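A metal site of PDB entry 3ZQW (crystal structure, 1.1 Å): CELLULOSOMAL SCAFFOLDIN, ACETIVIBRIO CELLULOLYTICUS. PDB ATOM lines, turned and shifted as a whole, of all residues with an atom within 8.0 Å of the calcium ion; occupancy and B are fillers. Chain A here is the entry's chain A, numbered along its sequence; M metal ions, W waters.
The side-chain amide oxygen of Asn 119 lies within hydrogen-bond range of the backbone NH of Ala 121, at 3.1 Å. The backbone carbonyl oxygen of Asp 50 is in hydrogen-bond range of the side-chain amino group of Lys 112.
Of the 21 residues printed, 5 come within 4 Å of the calcium ion.
The calcium ion is bound by OD2 of Asp 50 (2.3 Å), O of Asn 119 (2.3 Å), OD1 of Asp 123 (2.4 Å), OG1 of Thr 48 (2.4 Å), OD1 of Asp 122 (2.4 Å), water W1 (2.5 Å) and O of Thr 48 (2.5 Å).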
ATOM      1  N   ALA A  17      28.751  10.018   3.643  1.00  0.00           N
ATOM      2  CA  ALA A  17      28.418  10.193   5.062  1.00  0.00           C
ATOM      3  C   ALA A  17      29.576  10.801   5.835  1.00  0.00           C
ATOM      4  O   ALA A  17      29.405  11.794   6.532  1.00  0.00           O
ATOM      5  CB  ALA A  17      27.997   8.878   5.676  1.00  0.00           C
ATOM      6  N   ILE A  22      30.511  19.965   3.412  1.00  0.00           N
ATOM      7  CA  ILE A  22      29.100  19.864   3.121  1.00  0.00           C
ATOM      8  C   ILE A  22      28.854  20.794   1.931  1.00  0.00           C
ATOM      9  O   ILE A  22      29.441  21.879   1.837  1.00  0.00           O
ATOM     10  CB  ILE A  22      28.239  20.179   4.370  1.00  0.00           C
ATOM     11  CG1 ILE A  22      28.548  19.091   5.414  1.00  0.00           C
ATOM     12  CG2 ILE A  22      26.759  20.203   4.039  1.00  0.00           C
ATOM     13  CD1 ILE A  22      27.909  19.294   6.789  1.00  0.00           C
ATOM     14  N   TYR A  46      20.526  22.976   8.350  1.00  0.00           N
ATOM     15  CA  TYR A  46      20.641  22.484   9.724  1.00  0.00           C
ATOM     16  C   TYR A  46      21.414  21.170   9.776  1.00  0.00           C
ATOM     17  O   TYR A  46      21.193  20.265   8.952  1.00  0.00           O
ATOM     18  CB  TYR A  46      19.234  22.229  10.284  1.00  0.00           C
ATOM     19  CG  TYR A  46      18.392  23.489  10.411  1.00  0.00           C
ATOM     20  CD1 TYR A  46      18.491  24.286  11.536  1.00  0.00           C
ATOM     21  CD2 TYR A  46      17.539  23.890   9.396  1.00  0.00           C
ATOM     22  CE1 TYR A  46      17.752  25.427  11.687  1.00  0.00           C
ATOM     23  CE2 TYR A  46      16.773  25.041   9.531  1.00  0.00           C
ATOM     24  CZ  TYR A  46      16.887  25.809  10.671  1.00  0.00           C
ATOM     25  OH  TYR A  46      16.120  26.951  10.789  1.00  0.00           O
ATOM     26  N   PHE A  47      22.285  21.041  10.759  1.00  0.00           N
ATOM     27  CA  PHE A  47      23.164  19.884  10.814  1.00  0.00           C
ATOM     28  C   PHE A  47      23.680  19.677  12.231  1.00  0.00           C
ATOM     29  O   PHE A  47      23.530  20.542  13.095  1.00  0.00           O
ATOM     30  CB  PHE A  47      24.337  20.058   9.823  1.00  0.00           C
ATOM     31  CG  PHE A  47      25.245  21.226  10.110  1.00  0.00           C
ATOM     32  CD1 PHE A  47      24.930  22.526   9.747  1.00  0.00           C
ATOM     33  CD2 PHE A  47      26.476  21.018  10.731  1.00  0.00           C
ATOM     34  CE1 PHE A  47      25.784  23.587   9.991  1.00  0.00           C
ATOM     35  CE2 PHE A  47      27.347  22.069  10.980  1.00  0.00           C
ATOM     36  CZ  PHE A  47      27.000  23.367  10.597  1.00  0.00           C
ATOM     37  N   THR A  48      24.281  18.518  12.470  1.00  0.00           N
ATOM     38  CA  THR A  48      25.068  18.286  13.671  1.00  0.00           C
ATOM     39  C   THR A  48      26.537  18.374  13.264  1.00  0.00           C
ATOM     40  O   THR A  48      26.978  17.729  12.302  1.00  0.00           O
ATOM     41  CB  THR A  48      24.777  16.938  14.352  1.00  0.00           C
ATOM     42  OG1 THR A  48      25.142  15.887  13.472  1.00  0.00           O
ATOM     43  CG2 THR A  48      23.317  16.813  14.732  1.00  0.00           C
ATOM     44  N   VAL A  49      27.294  19.192  13.993  1.00  0.00           N
ATOM     45  CA  VAL A  49      28.645  19.513  13.571  1.00  0.00           C
ATOM     46  C   VAL A  49      29.647  18.378  13.709  1.00  0.00           C
ATOM     47  O   VAL A  49      30.649  18.374  13.002  1.00  0.00           O
ATOM     48  CB  VAL A  49      29.109  20.796  14.342  1.00  0.00           C
ATOM     49  CG1 VAL A  49      29.346  20.525  15.807  1.00  0.00           C
ATOM     50  CG2 VAL A  49      30.347  21.410  13.704  1.00  0.00           C
ATOM     51  N   ASP A  50      29.404  17.431  14.628  1.00  0.00           N
ATOM     52  CA  ASP A  50      30.321  16.304  14.834  1.00  0.00           C
ATOM     53  C   ASP A  50      31.734  16.778  15.155  1.00  0.00           C
ATOM     54  O   ASP A  50      32.715  16.409  14.505  1.00  0.00           O
ATOM     55  CB  ASP A  50      30.318  15.373  13.627  1.00  0.00           C
ATOM     56  CG  ASP A  50      28.987  14.738  13.399  1.00  0.00           C
ATOM     57  OD1 ASP A  50      28.534  14.025  14.330  1.00  0.00           O
ATOM     58  OD2 ASP A  50      28.385  14.917  12.329  1.00  0.00           O
ATOM     59  N   GLY A  51      31.808  17.586  16.219  1.00  0.00           N
ATOM     60  CA  GLY A  51      33.044  18.199  16.668  1.00  0.00           C
ATOM     61  C   GLY A  51      33.097  19.651  16.216  1.00  0.00           C
ATOM     62  O   GLY A  51      33.368  19.947  15.062  1.00  0.00           O
ATOM     63  N   GLY A  82      19.054  15.970  14.859  1.00  0.00           N
ATOM     64  CA  GLY A  82      19.610  16.324  13.579  1.00  0.00           C
ATOM     65  C   GLY A  82      20.174  17.725  13.478  1.00  0.00           C
ATOM     66  O   GLY A  82      20.639  18.096  12.398  1.00  0.00           O
ATOM     67  N   ALA A  83      20.129  18.516  14.546  1.00  0.00           N
ATOM     68  CA  ALA A  83      20.504  19.917  14.434  1.00  0.00           C
ATOM     69  C   ALA A  83      21.081  20.449  15.729  1.00  0.00           C
ATOM     70  O   ALA A  83      20.350  20.736  16.692  1.00  0.00           O
ATOM     71  CB  ALA A  83      19.290  20.744  14.028  1.00  0.00           C
ATOM     72  N   ASP A  84      22.390  20.640  15.752  1.00  0.00           N
ATOM     73  CA  ASP A  84      23.035  21.431  16.795  1.00  0.00           C
ATOM     74  C   ASP A  84      23.576  22.740  16.257  1.00  0.00           C
ATOM     75  O   ASP A  84      23.944  23.590  17.080  1.00  0.00           O
ATOM     76  CB  ASP A  84      24.055  20.650  17.628  1.00  0.00           C
ATOM     77  CG  ASP A  84      25.182  20.063  16.836  1.00  0.00           C
ATOM     78  OD1 ASP A  84      25.658  20.643  15.872  1.00  0.00           O
ATOM     79  OD2 ASP A  84      25.535  18.919  17.183  1.00  0.00           O
ATOM     80  N   LYS A 112      35.344  22.783   8.110  1.00  0.00           N
ATOM     81  CA  LYS A 112      35.988  23.167   9.357  1.00  0.00           C
ATOM     82  C   LYS A 112      37.388  23.678   9.092  1.00  0.00           C
ATOM     83  O   LYS A 112      38.053  23.300   8.125  1.00  0.00           O
ATOM     84  CB  LYS A 112      36.049  21.955  10.286  1.00  0.00           C
ATOM     85  CG  LYS A 112      34.688  21.398  10.618  1.00  0.00           C
ATOM     86  CD  LYS A 112      34.775  20.176  11.517  1.00  0.00           C
ATOM     87  CE  LYS A 112      33.420  19.538  11.642  1.00  0.00           C
ATOM     88  NZ  LYS A 112      33.407  18.386  12.578  1.00  0.00           N
ATOM     89  N   ASN A 117      36.372  15.794   9.781  1.00  0.00           N
ATOM     90  CA  ASN A 117      35.162  15.291   9.171  1.00  0.00           C
ATOM     91  C   ASN A 117      33.869  15.666   9.879  1.00  0.00           C
ATOM     92  O   ASN A 117      33.818  15.825  11.111  1.00  0.00           O
ATOM     93  CB  ASN A 117      35.191  13.776   9.040  1.00  0.00           C
ATOM     94  CG  ASN A 117      36.192  13.309   8.000  1.00  0.00           C
ATOM     95  OD1 ASN A 117      36.499  14.010   7.048  1.00  0.00           O
ATOM     96  ND2 ASN A 117      36.727  12.119   8.192  1.00  0.00           N
ATOM     97  N   TYR A 118      32.827  15.746   9.066  1.00  0.00           N
ATOM     98  CA  TYR A 118      31.427  15.701   9.447  1.00  0.00           C
ATOM     99  C   TYR A 118      30.896  14.279   9.240  1.00  0.00           C
ATOM    100  O   TYR A 118      31.425  13.524   8.421  1.00  0.00           O
ATOM    101  CB  TYR A 118      30.614  16.602   8.517  1.00  0.00           C
ATOM    102  CG  TYR A 118      30.950  18.072   8.573  1.00  0.00           C
ATOM    103  CD1 TYR A 118      30.435  18.881   9.555  1.00  0.00           C
ATOM    104  CD2 TYR A 118      31.761  18.654   7.624  1.00  0.00           C
ATOM    105  CE1 TYR A 118      30.705  20.251   9.588  1.00  0.00           C
ATOM    106  CE2 TYR A 118      32.046  20.005   7.644  1.00  0.00           C
ATOM    107  CZ  TYR A 118      31.500  20.817   8.614  1.00  0.00           C
ATOM    108  OH  TYR A 118      31.792  22.144   8.601  1.00  0.00           O
ATOM    109  N   ASN A 119      29.802  13.947   9.937  1.00  0.00           N
ATOM    110  CA  ASN A 119      28.917  12.845   9.580  1.00  0.00           C
ATOM    111  C   ASN A 119      27.644  13.436   8.996  1.00  0.00           C
ATOM    112  O   ASN A 119      26.826  13.991   9.731  1.00  0.00           O
ATOM    113  CB  ASN A 119      28.566  11.969  10.795  1.00  0.00           C
ATOM    114  CG  ASN A 119      27.505  10.967  10.474  1.00  0.00           C
ATOM    115  OD1 ASN A 119      27.386  10.542   9.324  1.00  0.00           O
ATOM    116  ND2 ASN A 119      26.719  10.582  11.465  1.00  0.00           N
ATOM    117  N   GLN A 120      27.475  13.370   7.682  1.00  0.00           N
ATOM    118  CA  GLN A 120      26.318  13.987   7.078  1.00  0.00           C
ATOM    119  C   GLN A 120      25.027  13.237   7.383  1.00  0.00           C
ATOM    120  O   GLN A 120      23.942  13.805   7.300  1.00  0.00           O
ATOM    121  CB  GLN A 120      26.468  14.096   5.553  1.00  0.00           C
ATOM    122  CG  GLN A 120      27.695  14.866   5.128  1.00  0.00           C
ATOM    123  CD  GLN A 120      27.504  15.471   3.755  1.00  0.00           C
ATOM    124  OE1 GLN A 120      26.839  16.489   3.616  1.00  0.00           O
ATOM    125  NE2 GLN A 120      28.062  14.815   2.736  1.00  0.00           N
ATOM    126  N   ALA A 121      25.140  11.931   7.681  1.00  0.00           N
ATOM    127  CA  ALA A 121      23.972  11.087   7.667  1.00  0.00           C
ATOM    128  C   ALA A 121      22.912  11.485   8.678  1.00  0.00           C
ATOM    129  O   ALA A 121      21.734  11.238   8.441  1.00  0.00           O
ATOM    130  CB  ALA A 121      24.379   9.643   7.897  1.00  0.00           C
ATOM    131  N   ASP A 122      23.324  12.080   9.792  1.00  0.00           N
ATOM    132  CA  ASP A 122      22.371  12.471  10.835  1.00  0.00           C
ATOM    133  C   ASP A 122      21.902  13.901  10.717  1.00  0.00           C
ATOM    134  O   ASP A 122      21.183  14.367  11.597  1.00  0.00           O
ATOM    135  CB  ASP A 122      22.939  12.239  12.229  1.00  0.00           C
ATOM    136  CG  ASP A 122      24.082  13.181  12.600  1.00  0.00           C
ATOM    137  OD1 ASP A 122      24.787  13.648  11.694  1.00  0.00           O
ATOM    138  OD2 ASP A 122      24.270  13.416  13.824  1.00  0.00           O
ATOM    139  N   ASP A 123      22.280  14.615   9.665  1.00  0.00           N
ATOM    140  CA  ASP A 123      21.952  16.028   9.606  1.00  0.00           C
ATOM    141  C   ASP A 123      20.518  16.253   9.155  1.00  0.00           C
ATOM    142  O   ASP A 123      20.070  15.707   8.154  1.00  0.00           O
ATOM    143  CB  ASP A 123      22.889  16.749   8.633  1.00  0.00           C
ATOM    144  CG  ASP A 123      24.332  16.773   9.121  1.00  0.00           C
ATOM    145  OD1 ASP A 123      24.551  16.578  10.332  1.00  0.00           O
ATOM    146  OD2 ASP A 123      25.221  16.993   8.268  1.00  0.00           O
ATOM    147  N   TYR A 124      19.806  17.115   9.870  1.00  0.00           N
ATOM    148  CA  TYR A 124      18.411  17.416   9.582  1.00  0.00           C
ATOM    149  C   TYR A 124      18.189  17.771   8.116  1.00  0.00           C
ATOM    150  O   TYR A 124      17.232  17.305   7.496  1.00  0.00           O
ATOM    151  CB  TYR A 124      17.948  18.555  10.488  1.00  0.00           C
ATOM    152  CG  TYR A 124      16.539  19.012  10.333  1.00  0.00           C
ATOM    153  CD1 TYR A 124      16.186  20.026   9.467  1.00  0.00           C
ATOM    154  CD2 TYR A 124      15.551  18.467  11.137  1.00  0.00           C
ATOM    155  CE1 TYR A 124      14.893  20.479   9.364  1.00  0.00           C
ATOM    156  CE2 TYR A 124      14.248  18.915  11.060  1.00  0.00           C
ATOM    157  CZ  TYR A 124      13.915  19.908  10.158  1.00  0.00           C
ATOM    158  OH  TYR A 124      12.595  20.330  10.085  1.00  0.00           O
ATOM    159  N   PHE A 126      20.197  17.196   5.439  1.00  0.00           N
ATOM    160  CA  PHE A 126      20.892  16.416   4.433  1.00  0.00           C
ATOM    161  C   PHE A 126      19.941  15.550   3.649  1.00  0.00           C
ATOM    162  O   PHE A 126      19.106  14.838   4.216  1.00  0.00           O
ATOM    163  CB  PHE A 126      21.926  15.521   5.133  1.00  0.00           C
ATOM    164  CG  PHE A 126      22.731  14.625   4.215  1.00  0.00           C
ATOM    165  CD1 PHE A 126      23.584  15.156   3.257  1.00  0.00           C
ATOM    166  CD2 PHE A 126      22.692  13.247   4.378  1.00  0.00           C
ATOM    167  CE1 PHE A 126      24.357  14.339   2.459  1.00  0.00           C
ATOM    168  CE2 PHE A 126      23.481  12.419   3.584  1.00  0.00           C
ATOM    169  CZ  PHE A 126      24.310  12.966   2.619  1.00  0.00           C
HETATM  170 CA    CA M   1      26.321  15.496  11.443  1.00  0.00          CA
HETATM  171  O   HOH W   1      27.507  16.806   9.705  1.00  0.00           O
